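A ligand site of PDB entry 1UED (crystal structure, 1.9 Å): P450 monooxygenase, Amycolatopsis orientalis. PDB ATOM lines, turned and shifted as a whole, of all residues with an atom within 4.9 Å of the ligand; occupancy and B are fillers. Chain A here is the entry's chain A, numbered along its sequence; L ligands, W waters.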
ATOM      1  N   LEU A  68      27.412  26.757 -11.273  1.00  0.00           N
ATOM      2  CA  LEU A  68      26.283  25.833 -11.087  1.00  0.00           C
ATOM      3  C   LEU A  68      25.319  25.935 -12.282  1.00  0.00           C
ATOM      4  O   LEU A  68      24.810  24.936 -12.745  1.00  0.00           O
ATOM      5  CB  LEU A  68      25.514  26.131  -9.765  1.00  0.00           C
ATOM      6  CG  LEU A  68      26.072  25.662  -8.415  1.00  0.00           C
ATOM      7  CD1 LEU A  68      25.084  26.057  -7.338  1.00  0.00           C
ATOM      8  CD2 LEU A  68      26.285  24.147  -8.385  1.00  0.00           C
ATOM      9  N   ILE A  97      18.615  12.094 -12.996  1.00  0.00           N
ATOM     10  CA  ILE A  97      18.510  13.417 -13.600  1.00  0.00           C
ATOM     11  C   ILE A  97      19.601  14.454 -13.303  1.00  0.00           C
ATOM     12  O   ILE A  97      19.961  15.245 -14.201  1.00  0.00           O
ATOM     13  CB  ILE A  97      17.106  14.028 -13.276  1.00  0.00           C
ATOM     14  CG1 ILE A  97      16.875  15.294 -14.107  1.00  0.00           C
ATOM     15  CG2 ILE A  97      16.986  14.330 -11.758  1.00  0.00           C
ATOM     16  CD1 ILE A  97      15.417  15.757 -14.089  1.00  0.00           C
ATOM     17  N   SER A  98      20.126  14.461 -12.077  1.00  0.00           N
ATOM     18  CA  SER A  98      21.164  15.445 -11.715  1.00  0.00           C
ATOM     19  C   SER A  98      22.460  15.219 -12.518  1.00  0.00           C
ATOM     20  O   SER A  98      23.278  16.149 -12.676  1.00  0.00           O
ATOM     21  CB  SER A  98      21.473  15.400 -10.213  1.00  0.00           C
ATOM     22  OG  SER A  98      22.224  14.246  -9.871  1.00  0.00           O
ATOM     23  N   HIS A 105      18.643  15.817 -20.218  1.00  0.00           N
ATOM     24  CA  HIS A 105      18.186  16.361 -18.936  1.00  0.00           C
ATOM     25  C   HIS A 105      16.804  16.991 -19.069  1.00  0.00           C
ATOM     26  O   HIS A 105      15.917  16.805 -18.223  1.00  0.00           O
ATOM     27  CB  HIS A 105      19.209  17.421 -18.398  1.00  0.00           C
ATOM     28  CG  HIS A 105      18.611  18.112 -17.158  1.00  0.00           C
ATOM     29  ND1 HIS A 105      17.947  19.318 -17.210  1.00  0.00           N
ATOM     30  CD2 HIS A 105      18.528  17.696 -15.872  1.00  0.00           C
ATOM     31  CE1 HIS A 105      17.459  19.603 -16.012  1.00  0.00           C
ATOM     32  NE2 HIS A 105      17.801  18.638 -15.181  1.00  0.00           N
ATOM     33  N   ARG A 109      13.497  16.258 -16.946  1.00  0.00           N
ATOM     34  CA  ARG A 109      13.037  17.365 -16.103  1.00  0.00           C
ATOM     35  C   ARG A 109      11.549  17.651 -16.419  1.00  0.00           C
ATOM     36  O   ARG A 109      10.708  17.822 -15.511  1.00  0.00           O
ATOM     37  CB  ARG A 109      13.885  18.615 -16.379  1.00  0.00           C
ATOM     38  CG  ARG A 109      13.493  19.848 -15.533  1.00  0.00           C
ATOM     39  CD  ARG A 109      13.879  19.683 -14.059  1.00  0.00           C
ATOM     40  NE  ARG A 109      13.455  20.840 -13.244  1.00  0.00           N
ATOM     41  CZ  ARG A 109      14.154  21.317 -12.218  1.00  0.00           C
ATOM     42  NH1 ARG A 109      15.285  20.736 -11.871  1.00  0.00           N
ATOM     43  NH2 ARG A 109      13.713  22.368 -11.520  1.00  0.00           N
ATOM     44  N   PHE A 116       5.415  18.450  -9.186  1.00  0.00           N
ATOM     45  CA  PHE A 116       5.928  19.283  -8.103  1.00  0.00           C
ATOM     46  C   PHE A 116       5.380  20.682  -7.995  1.00  0.00           C
ATOM     47  O   PHE A 116       5.950  21.528  -7.292  1.00  0.00           O
ATOM     48  CB  PHE A 116       7.461  19.347  -8.227  1.00  0.00           C
ATOM     49  CG  PHE A 116       8.139  18.098  -7.745  1.00  0.00           C
ATOM     50  CD1 PHE A 116       8.411  17.909  -6.393  1.00  0.00           C
ATOM     51  CD2 PHE A 116       8.484  17.098  -8.636  1.00  0.00           C
ATOM     52  CE1 PHE A 116       9.005  16.748  -5.944  1.00  0.00           C
ATOM     53  CE2 PHE A 116       9.073  15.938  -8.200  1.00  0.00           C
ATOM     54  CZ  PHE A 116       9.347  15.759  -6.848  1.00  0.00           C
ATOM     55  N   LEU A 161       8.609  11.118   1.351  1.00  0.00           N
ATOM     56  CA  LEU A 161       8.998  10.605   0.040  1.00  0.00           C
ATOM     57  C   LEU A 161       8.122   9.443  -0.354  1.00  0.00           C
ATOM     58  O   LEU A 161       7.728   9.324  -1.515  1.00  0.00           O
ATOM     59  CB  LEU A 161      10.468  10.171   0.042  1.00  0.00           C
ATOM     60  CG  LEU A 161      11.288  10.913  -1.007  1.00  0.00           C
ATOM     61  CD1 LEU A 161      10.896  10.431  -2.439  1.00  0.00           C
ATOM     62  CD2 LEU A 161      11.004  12.418  -0.867  1.00  0.00           C
ATOM     63  N   LEU A 164       4.882  10.817  -1.655  1.00  0.00           N
ATOM     64  CA  LEU A 164       5.070  11.420  -2.957  1.00  0.00           C
ATOM     65  C   LEU A 164       5.104  10.339  -4.052  1.00  0.00           C
ATOM     66  O   LEU A 164       4.449  10.488  -5.093  1.00  0.00           O
ATOM     67  CB  LEU A 164       6.388  12.188  -2.976  1.00  0.00           C
ATOM     68  CG  LEU A 164       6.801  12.769  -4.324  1.00  0.00           C
ATOM     69  CD1 LEU A 164       5.916  13.965  -4.666  1.00  0.00           C
ATOM     70  CD2 LEU A 164       8.264  13.170  -4.250  1.00  0.00           C
ATOM     71  N   ALA A 241      16.609   8.952  -7.710  1.00  0.00           N
ATOM     72  CA  ALA A 241      17.010  10.349  -7.685  1.00  0.00           C
ATOM     73  C   ALA A 241      16.207  11.145  -6.664  1.00  0.00           C
ATOM     74  O   ALA A 241      16.764  11.976  -5.941  1.00  0.00           O
ATOM     75  CB  ALA A 241      16.845  10.965  -9.071  1.00  0.00           C
ATOM     76  N   LEU A 242      14.885  10.906  -6.608  1.00  0.00           N
ATOM     77  CA  LEU A 242      14.020  11.602  -5.645  1.00  0.00           C
ATOM     78  C   LEU A 242      14.302  11.162  -4.226  1.00  0.00           C
ATOM     79  O   LEU A 242      14.286  11.997  -3.298  1.00  0.00           O
ATOM     80  CB  LEU A 242      12.519  11.386  -5.989  1.00  0.00           C
ATOM     81  CG  LEU A 242      12.135  12.022  -7.317  1.00  0.00           C
ATOM     82  CD1 LEU A 242      10.688  11.596  -7.724  1.00  0.00           C
ATOM     83  CD2 LEU A 242      12.274  13.551  -7.182  1.00  0.00           C
ATOM     84  N   GLY A 245      17.634  12.691  -3.445  1.00  0.00           N
ATOM     85  CA  GLY A 245      17.535  14.137  -3.337  1.00  0.00           C
ATOM     86  C   GLY A 245      16.599  14.694  -2.269  1.00  0.00           C
ATOM     87  O   GLY A 245      16.791  15.835  -1.803  1.00  0.00           O
ATOM     88  N   GLY A 246      15.633  13.902  -1.811  1.00  0.00           N
ATOM     89  CA  GLY A 246      14.690  14.464  -0.865  1.00  0.00           C
ATOM     90  C   GLY A 246      14.581  13.958   0.535  1.00  0.00           C
ATOM     91  O   GLY A 246      14.066  14.674   1.392  1.00  0.00           O
ATOM     92  N   THR A 249      17.887  15.439   2.732  1.00  0.00           N
ATOM     93  CA  THR A 249      17.870  16.903   2.705  1.00  0.00           C
ATOM     94  C   THR A 249      16.775  17.439   3.624  1.00  0.00           C
ATOM     95  O   THR A 249      16.998  18.358   4.407  1.00  0.00           O
ATOM     96  CB  THR A 249      17.597  17.447   1.314  1.00  0.00           C
ATOM     97  OG1 THR A 249      16.437  16.797   0.777  1.00  0.00           O
ATOM     98  CG2 THR A 249      18.791  17.228   0.409  1.00  0.00           C
ATOM     99  N   VAL A 250      15.567  16.880   3.495  1.00  0.00           N
ATOM    100  CA  VAL A 250      14.491  17.313   4.373  1.00  0.00           C
ATOM    101  C   VAL A 250      14.856  16.974   5.827  1.00  0.00           C
ATOM    102  O   VAL A 250      14.684  17.793   6.713  1.00  0.00           O
ATOM    103  CB  VAL A 250      13.118  16.635   4.013  1.00  0.00           C
ATOM    104  CG1 VAL A 250      12.092  16.867   5.147  1.00  0.00           C
ATOM    105  CG2 VAL A 250      12.573  17.269   2.693  1.00  0.00           C
ATOM    106  N   MET A 253      17.387  19.481   6.954  1.00  0.00           N
ATOM    107  CA  MET A 253      16.825  20.799   7.231  1.00  0.00           C
ATOM    108  C   MET A 253      16.023  20.801   8.526  1.00  0.00           C
ATOM    109  O   MET A 253      16.012  21.781   9.270  1.00  0.00           O
ATOM    110  CB  MET A 253      15.932  21.269   6.074  1.00  0.00           C
ATOM    111  CG  MET A 253      16.741  21.849   4.877  1.00  0.00           C
ATOM    112  SD  MET A 253      17.845  23.249   5.353  1.00  0.00           S
ATOM    113  CE  MET A 253      16.783  24.297   6.230  1.00  0.00           C
ATOM    114  N   VAL A 286      17.398  27.738   4.944  1.00  0.00           N
ATOM    115  CA  VAL A 286      18.035  27.042   3.826  1.00  0.00           C
ATOM    116  C   VAL A 286      19.312  27.802   3.430  1.00  0.00           C
ATOM    117  O   VAL A 286      20.345  27.178   3.213  1.00  0.00           O
ATOM    118  CB  VAL A 286      17.094  26.923   2.579  1.00  0.00           C
ATOM    119  CG1 VAL A 286      17.901  26.386   1.322  1.00  0.00           C
ATOM    120  CG2 VAL A 286      15.961  25.926   2.915  1.00  0.00           C
ATOM    121  N   PRO A 291      22.341  22.337   3.681  1.00  0.00           N
ATOM    122  CA  PRO A 291      22.695  20.915   3.928  1.00  0.00           C
ATOM    123  C   PRO A 291      23.301  20.213   2.714  1.00  0.00           C
ATOM    124  O   PRO A 291      24.100  19.264   2.866  1.00  0.00           O
ATOM    125  CB  PRO A 291      21.362  20.316   4.438  1.00  0.00           C
ATOM    126  CG  PRO A 291      20.311  21.135   3.735  1.00  0.00           C
ATOM    127  CD  PRO A 291      20.894  22.565   3.861  1.00  0.00           C
ATOM    128  N   VAL A 292      22.935  20.650   1.501  1.00  0.00           N
ATOM    129  CA  VAL A 292      23.583  20.145   0.301  1.00  0.00           C
ATOM    130  C   VAL A 292      24.737  21.139   0.187  1.00  0.00           C
ATOM    131  O   VAL A 292      24.676  22.114  -0.557  1.00  0.00           O
ATOM    132  CB  VAL A 292      22.703  20.186  -0.951  1.00  0.00           C
ATOM    133  CG1 VAL A 292      23.479  19.723  -2.188  1.00  0.00           C
ATOM    134  CG2 VAL A 292      21.458  19.333  -0.732  1.00  0.00           C
ATOM    135  N   PRO A 295      27.193  20.056  -4.089  1.00  0.00           N
ATOM    136  CA  PRO A 295      26.489  19.195  -5.052  1.00  0.00           C
ATOM    137  C   PRO A 295      27.503  18.465  -5.966  1.00  0.00           C
ATOM    138  O   PRO A 295      28.746  18.523  -5.762  1.00  0.00           O
ATOM    139  CB  PRO A 295      25.606  20.188  -5.821  1.00  0.00           C
ATOM    140  CG  PRO A 295      26.466  21.481  -5.821  1.00  0.00           C
ATOM    141  CD  PRO A 295      27.061  21.498  -4.400  1.00  0.00           C
ATOM    142  N   ASN A 296      26.982  17.806  -6.985  1.00  0.00           N
ATOM    143  CA  ASN A 296      27.834  17.093  -7.927  1.00  0.00           C
ATOM    144  C   ASN A 296      28.932  17.966  -8.460  1.00  0.00           C
ATOM    145  O   ASN A 296      28.708  19.109  -8.817  1.00  0.00           O
ATOM    146  CB  ASN A 296      27.072  16.604  -9.167  1.00  0.00           C
ATOM    147  CG  ASN A 296      26.182  15.399  -8.892  1.00  0.00           C
ATOM    148  OD1 ASN A 296      26.479  14.563  -8.077  1.00  0.00           O
ATOM    149  ND2 ASN A 296      25.072  15.322  -9.604  1.00  0.00           N
ATOM    150  N   ARG A 298      31.492  19.705 -10.908  1.00  0.00           N
ATOM    151  CA  ARG A 298      31.291  20.079 -12.299  1.00  0.00           C
ATOM    152  C   ARG A 298      32.569  19.787 -13.076  1.00  0.00           C
ATOM    153  O   ARG A 298      33.644  20.266 -12.702  1.00  0.00           O
ATOM    154  CB  ARG A 298      30.931  21.573 -12.420  1.00  0.00           C
ATOM    155  CG  ARG A 298      29.418  21.823 -12.589  1.00  0.00           C
ATOM    156  CD  ARG A 298      28.572  21.423 -11.392  1.00  0.00           C
ATOM    157  NE  ARG A 298      27.169  21.869 -11.577  1.00  0.00           N
ATOM    158  CZ  ARG A 298      26.140  21.449 -10.828  1.00  0.00           C
ATOM    159  NH1 ARG A 298      26.335  20.570  -9.848  1.00  0.00           N
ATOM    160  NH2 ARG A 298      24.904  21.857 -11.097  1.00  0.00           N
ATOM    161  N   ILE A 321      28.097  25.416  -1.945  1.00  0.00           N
ATOM    162  CA  ILE A 321      26.854  26.166  -1.780  1.00  0.00           C
ATOM    163  C   ILE A 321      26.873  26.775  -0.383  1.00  0.00           C
ATOM    164  O   ILE A 321      26.499  27.933  -0.217  1.00  0.00           O
ATOM    165  CB  ILE A 321      25.628  25.200  -1.965  1.00  0.00           C
ATOM    166  CG1 ILE A 321      25.500  24.883  -3.460  1.00  0.00           C
ATOM    167  CG2 ILE A 321      24.392  25.754  -1.324  1.00  0.00           C
ATOM    168  CD1 ILE A 321      24.287  23.987  -3.824  1.00  0.00           C
ATOM    169  N   VAL A 347      21.909  30.390  -3.144  1.00  0.00           N
ATOM    170  CA  VAL A 347      22.025  29.181  -3.984  1.00  0.00           C
ATOM    171  C   VAL A 347      21.777  27.887  -3.177  1.00  0.00           C
ATOM    172  O   VAL A 347      22.242  26.814  -3.562  1.00  0.00           O
ATOM    173  CB  VAL A 347      23.436  29.075  -4.649  1.00  0.00           C
ATOM    174  CG1 VAL A 347      23.616  30.188  -5.697  1.00  0.00           C
ATOM    175  CG2 VAL A 347      24.574  29.184  -3.567  1.00  0.00           C
ATOM    176  N   GLY A 348      21.036  28.005  -2.084  1.00  0.00           N
ATOM    177  CA  GLY A 348      20.721  26.838  -1.269  1.00  0.00           C
ATOM    178  C   GLY A 348      20.020  25.695  -2.001  1.00  0.00           C
ATOM    179  O   GLY A 348      20.220  24.516  -1.667  1.00  0.00           O
ATOM    180  N   PHE A 349      19.155  26.042  -2.956  1.00  0.00           N
ATOM    181  CA  PHE A 349      18.454  25.050  -3.799  1.00  0.00           C
ATOM    182  C   PHE A 349      19.125  24.929  -5.163  1.00  0.00           C
ATOM    183  O   PHE A 349      18.556  24.352  -6.115  1.00  0.00           O
ATOM    184  CB  PHE A 349      16.999  25.470  -3.986  1.00  0.00           C
ATOM    185  CG  PHE A 349      16.141  25.179  -2.791  1.00  0.00           C
ATOM    186  CD1 PHE A 349      15.911  23.857  -2.381  1.00  0.00           C
ATOM    187  CD2 PHE A 349      15.545  26.228  -2.072  1.00  0.00           C
ATOM    188  CE1 PHE A 349      15.063  23.590  -1.250  1.00  0.00           C
ATOM    189  CE2 PHE A 349      14.713  25.967  -0.947  1.00  0.00           C
ATOM    190  CZ  PHE A 349      14.481  24.644  -0.560  1.00  0.00           C
ATOM    191  N   GLY A 350      20.328  25.476  -5.281  1.00  0.00           N
ATOM    192  CA  GLY A 350      21.038  25.431  -6.547  1.00  0.00           C
ATOM    193  C   GLY A 350      20.730  26.624  -7.437  1.00  0.00           C
ATOM    194  O   GLY A 350      20.248  27.675  -6.968  1.00  0.00           O
ATOM    195  N   ILE A 353      19.676  24.826 -14.702  1.00  0.00           N
ATOM    196  CA  ILE A 353      18.826  23.709 -15.072  1.00  0.00           C
ATOM    197  C   ILE A 353      18.598  22.666 -13.967  1.00  0.00           C
ATOM    198  O   ILE A 353      17.564  22.040 -13.938  1.00  0.00           O
ATOM    199  CB  ILE A 353      19.326  22.952 -16.368  1.00  0.00           C
ATOM    200  CG1 ILE A 353      20.643  22.255 -16.096  1.00  0.00           C
ATOM    201  CG2 ILE A 353      19.417  23.926 -17.574  1.00  0.00           C
ATOM    202  CD1 ILE A 353      21.114  21.356 -17.282  1.00  0.00           C
ATOM    203  N   HIS A 354      19.565  22.474 -13.067  1.00  0.00           N
ATOM    204  CA  HIS A 354      19.393  21.485 -12.005  1.00  0.00           C
ATOM    205  C   HIS A 354      18.773  22.079 -10.725  1.00  0.00           C
ATOM    206  O   HIS A 354      18.687  21.386  -9.715  1.00  0.00           O
ATOM    207  CB  HIS A 354      20.760  20.796 -11.685  1.00  0.00           C
ATOM    208  CG  HIS A 354      21.317  20.008 -12.838  1.00  0.00           C
ATOM    209  ND1 HIS A 354      20.758  18.817 -13.264  1.00  0.00           N
ATOM    210  CD2 HIS A 354      22.378  20.236 -13.639  1.00  0.00           C
ATOM    211  CE1 HIS A 354      21.458  18.347 -14.291  1.00  0.00           C
ATOM    212  NE2 HIS A 354      22.454  19.195 -14.533  1.00  0.00           N
ATOM    213  N   TYR A 355      18.320  23.335 -10.763  1.00  0.00           N
ATOM    214  CA  TYR A 355      17.672  23.953  -9.593  1.00  0.00           C
ATOM    215  C   TYR A 355      16.693  22.944  -8.953  1.00  0.00           C
ATOM    216  O   TYR A 355      15.860  22.360  -9.643  1.00  0.00           O
ATOM    217  CB  TYR A 355      16.904  25.224 -10.003  1.00  0.00           C
ATOM    218  CG  TYR A 355      16.278  25.940  -8.842  1.00  0.00           C
ATOM    219  CD1 TYR A 355      16.974  26.914  -8.137  1.00  0.00           C
ATOM    220  CD2 TYR A 355      14.978  25.630  -8.422  1.00  0.00           C
ATOM    221  CE1 TYR A 355      16.404  27.577  -7.043  1.00  0.00           C
ATOM    222  CE2 TYR A 355      14.393  26.276  -7.331  1.00  0.00           C
ATOM    223  CZ  TYR A 355      15.096  27.247  -6.645  1.00  0.00           C
ATOM    224  OH  TYR A 355      14.502  27.885  -5.566  1.00  0.00           O
ATOM    225  N   CYS A 356      16.772  22.772  -7.639  1.00  0.00           N
ATOM    226  CA  CYS A 356      15.956  21.768  -6.932  1.00  0.00           C
ATOM    227  C   CYS A 356      14.518  21.627  -7.459  1.00  0.00           C
ATOM    228  O   CYS A 356      13.750  22.576  -7.440  1.00  0.00           O
ATOM    229  CB  CYS A 356      15.945  22.066  -5.439  1.00  0.00           C
ATOM    230  SG  CYS A 356      15.059  20.758  -4.555  1.00  0.00           S
ATOM    231  N   VAL A 357      14.178  20.436  -7.958  1.00  0.00           N
ATOM    232  CA  VAL A 357      12.821  20.218  -8.466  1.00  0.00           C
ATOM    233  C   VAL A 357      11.855  20.108  -7.286  1.00  0.00           C
ATOM    234  O   VAL A 357      10.640  20.338  -7.431  1.00  0.00           O
ATOM    235  CB  VAL A 357      12.791  18.917  -9.342  1.00  0.00           C
ATOM    236  CG1 VAL A 357      12.879  17.647  -8.463  1.00  0.00           C
ATOM    237  CG2 VAL A 357      11.595  18.901 -10.213  1.00  0.00           C
ATOM    238  N   GLY A 358      12.424  19.815  -6.111  1.00  0.00           N
ATOM    239  CA  GLY A 358      11.607  19.679  -4.906  1.00  0.00           C
ATOM    240  C   GLY A 358      11.522  20.903  -3.993  1.00  0.00           C
ATOM    241  O   GLY A 358      10.944  20.800  -2.913  1.00  0.00           O
ATOM    242  N   LEU A 361       8.039  21.870  -2.520  1.00  0.00           N
ATOM    243  CA  LEU A 361       7.598  20.867  -1.551  1.00  0.00           C
ATOM    244  C   LEU A 361       8.392  21.025  -0.244  1.00  0.00           C
ATOM    245  O   LEU A 361       7.841  20.979   0.868  1.00  0.00           O
ATOM    246  CB  LEU A 361       7.821  19.462  -2.105  1.00  0.00           C
ATOM    247  CG  LEU A 361       7.645  18.289  -1.164  1.00  0.00           C
ATOM    248  CD1 LEU A 361       6.202  18.231  -0.623  1.00  0.00           C
ATOM    249  CD2 LEU A 361       7.994  17.001  -1.919  1.00  0.00           C
ATOM    250  N   ALA A 362       9.711  21.177  -0.384  1.00  0.00           N
ATOM    251  CA  ALA A 362      10.541  21.328   0.829  1.00  0.00           C
ATOM    252  C   ALA A 362      10.112  22.538   1.612  1.00  0.00           C
ATOM    253  O   ALA A 362       9.977  22.472   2.843  1.00  0.00           O
ATOM    254  CB  ALA A 362      12.033  21.443   0.457  1.00  0.00           C
ATOM    255  N   MET A 365       6.772  21.642   3.450  1.00  0.00           N
ATOM    256  CA  MET A 365       6.947  20.670   4.524  1.00  0.00           C
ATOM    257  C   MET A 365       7.720  21.227   5.702  1.00  0.00           C
ATOM    258  O   MET A 365       7.370  20.972   6.856  1.00  0.00           O
ATOM    259  CB  MET A 365       7.675  19.423   4.025  1.00  0.00           C
ATOM    260  CG  MET A 365       6.917  18.669   2.971  1.00  0.00           C
ATOM    261  SD  MET A 365       7.592  17.009   2.856  1.00  0.00           S
ATOM    262  CE  MET A 365       9.127  17.287   2.245  1.00  0.00           C
ATOM    263  N   LEU A 366       8.771  22.001   5.406  1.00  0.00           N
ATOM    264  CA  LEU A 366       9.569  22.596   6.469  1.00  0.00           C
ATOM    265  C   LEU A 366       8.729  23.622   7.277  1.00  0.00           C
ATOM    266  O   LEU A 366       8.789  23.631   8.521  1.00  0.00           O
ATOM    267  CB  LEU A 366      10.864  23.234   5.885  1.00  0.00           C
ATOM    268  CG  LEU A 366      11.837  22.228   5.260  1.00  0.00           C
ATOM    269  CD1 LEU A 366      13.065  22.984   4.707  1.00  0.00           C
ATOM    270  CD2 LEU A 366      12.293  21.155   6.311  1.00  0.00           C
HETATM  271  C1  LIG L   1      18.498  19.278  -6.988  1.00  0.00           C
HETATM  272  C2  LIG L   1      18.927  21.124  -2.573  1.00  0.00           C
HETATM  273  C3  LIG L   1      14.810  18.950  -1.127  1.00  0.00           C
HETATM  274  C4  LIG L   1      14.911  16.519  -5.289  1.00  0.00           C
HETATM  275  C5  LIG L   1      18.952  20.086  -5.944  1.00  0.00           C
HETATM  276  C6  LIG L   1      20.163  20.901  -5.911  1.00  0.00           C
HETATM  277  C7  LIG L   1      20.274  21.377  -4.674  1.00  0.00           C
HETATM  278  C8  LIG L   1      19.160  20.807  -3.908  1.00  0.00           C
HETATM  279  C9  LIG L   1      21.463  22.098  -4.020  1.00  0.00           C
HETATM  280  C10 LIG L   1      21.116  21.269  -7.064  1.00  0.00           C
HETATM  281  C11 LIG L   1      22.021  20.074  -7.327  1.00  0.00           C
HETATM  282  C12 LIG L   1      23.054  20.336  -8.423  1.00  0.00           C
HETATM  283  O1  LIG L   1      23.869  19.421  -8.701  1.00  0.00           O
HETATM  284  O2  LIG L   1      23.006  21.455  -8.983  1.00  0.00           O
HETATM  285  C13 LIG L   1      17.875  20.675  -1.731  1.00  0.00           C
HETATM  286  C14 LIG L   1      17.597  21.164  -0.408  1.00  0.00           C
HETATM  287  C15 LIG L   1      16.429  20.515  -0.035  1.00  0.00           C
HETATM  288  C16 LIG L   1      16.033  19.646  -1.102  1.00  0.00           C
HETATM  289  C17 LIG L   1      18.392  22.230   0.424  1.00  0.00           C
HETATM  290  C18 LIG L   1      15.627  20.637   1.154  1.00  0.00           C
HETATM  291  C19 LIG L   1      15.485  21.896   1.622  1.00  0.00           C
HETATM  292  C20 LIG L   1      14.474  18.124  -2.202  1.00  0.00           C
HETATM  293  C21 LIG L   1      13.326  17.218  -2.176  1.00  0.00           C
HETATM  294  C22 LIG L   1      13.369  16.500  -3.307  1.00  0.00           C
HETATM  295  C23 LIG L   1      14.510  17.040  -4.080  1.00  0.00           C
HETATM  296  C24 LIG L   1      12.231  17.271  -1.058  1.00  0.00           C
HETATM  297  C25 LIG L   1      12.562  15.408  -3.741  1.00  0.00           C
HETATM  298  C26 LIG L   1      11.213  15.381  -3.601  1.00  0.00           C
HETATM  299  C27 LIG L   1      16.010  16.935  -6.077  1.00  0.00           C
HETATM  300  C28 LIG L   1      16.320  16.449  -7.367  1.00  0.00           C
HETATM  301  C29 LIG L   1      17.265  17.283  -7.936  1.00  0.00           C
HETATM  302  C30 LIG L   1      17.499  18.316  -6.932  1.00  0.00           C
HETATM  303  C31 LIG L   1      15.778  15.158  -7.964  1.00  0.00           C
HETATM  304  C32 LIG L   1      17.899  17.152  -9.301  1.00  0.00           C
HETATM  305  C33 LIG L   1      17.159  18.132 -10.243  1.00  0.00           C
HETATM  306  C34 LIG L   1      17.744  18.160 -11.674  1.00  0.00           C
HETATM  307  O3  LIG L   1      18.864  17.668 -11.871  1.00  0.00           O
HETATM  308  O4  LIG L   1      17.068  18.701 -12.595  1.00  0.00           O
HETATM  309  N1  LIG L   1      18.400  20.046  -4.714  1.00  0.00           N
HETATM  310  N2  LIG L   1      16.872  19.793  -2.162  1.00  0.00           N
HETATM  311  N3  LIG L   1      15.127  18.050  -3.376  1.00  0.00           N
HETATM  312  N4  LIG L   1      16.769  18.035  -5.768  1.00  0.00           N
HETATM  313 FE1  LIG L   1      16.726  19.093  -4.029  1.00  0.00          FE
HETATM  314  O   HOH W   1      18.288  17.329  -3.233  1.00  0.00           O
HETATM  315  O   HOH W   2      24.384  18.032 -10.883  1.00  0.00           O
HETATM  316  O   HOH W   3      21.906  23.696  -9.524  1.00  0.00           O
HETATM  317  O   HOH W   4      24.188  17.370  -6.943  1.00  0.00           O
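SG of Cys 356 is bound to FE1 of the ligand (2.4 Å). The guanidinium group (NH1) of Arg 109 is in salt-bridge range of an oxygen (O4) of the ligand (2.8 Å). An oxygen (O3) of the ligand is in hydrogen-bond range of a ring nitrogen (ND1) of His 354 (2.6 Å). O4 of the ligand is in hydrogen-bond range of NE2 of His 105 (2.7 Å). The guanidinium group (NH2) of Arg 298 is in salt-bridge range of an oxygen (O2) of the ligand, 2.9 Å away. An oxygen (O3) of the ligand lies close to the backbone NH (N) of Ser 98 (3.5 Å).
N of Cys 356 sits at hydrogen-bond distance from O of Phe 349 (2.8 Å). The side-chain hydroxyl (OG) of Ser 98 is in hydrogen-bond range of the side-chain amide nitrogen (ND2) of Asn 296. N of Gly 358 lies close to SG of Cys 356 (3.2 Å). The guanidinium group (NH1) of Arg 109 lies within hydrogen-bond range of the backbone carbonyl oxygen (O) of Tyr 355 (2.8 Å). OG1 of Thr 249 sits at hydrogen-bond distance from O of Gly 245, at 2.8 Å. O of Ile 353 sits at hydrogen-bond distance from NH1 of Arg 109 (3.3 Å). The backbone carbonyl oxygen (O) of Gly 246 lies within hydrogen-bond range of the side-chain hydroxyl (OG1) of Thr 249 (3.2 Å). The guanidinium group (NH1) of Arg 298 lies within hydrogen-bond range of the backbone carbonyl oxygen (O) of Asn 296.
The backbone carbonyl oxygen of Gly 245 sits close to a nitrogen (N3) of the ligand, 3.2 Å away. Residues that only touch the ligand: Ile 97, Phe 116, Leu 164, Ala 241, Leu 242, Gly 246, Thr 249, Val 250, Met 253, Pro 291, Val 292, Pro 295, Asn 296, Ile 321, Gly 348, Phe 349, Gly 350, Ile 353, Val 357, Gly 358, Leu 361 and Ala 362. Hydrophobic or aromatic side chains within 4 Å of the ligand: Ile 97, His 105, Phe 116, Leu 164, Leu 242, Val 250, Met 253, Pro 291, Val 292, Pro 295, Ile 321, Phe 349, His 354, Val 357, Leu 361 and Ala 362. Of the 36 residues printed, 29 come within 4 Å of the ligand.
Water W2 lies within hydrogen-bond range of an oxygen (O1) of the ligand, the backbone carbonyl oxygen (O) of Ser 98, the side-chain amide nitrogen (ND2) of Asn 296 and the guanidinium group (NH1) of Arg 298. Water W4 bridges O1 of the ligand and N of Asn 296.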
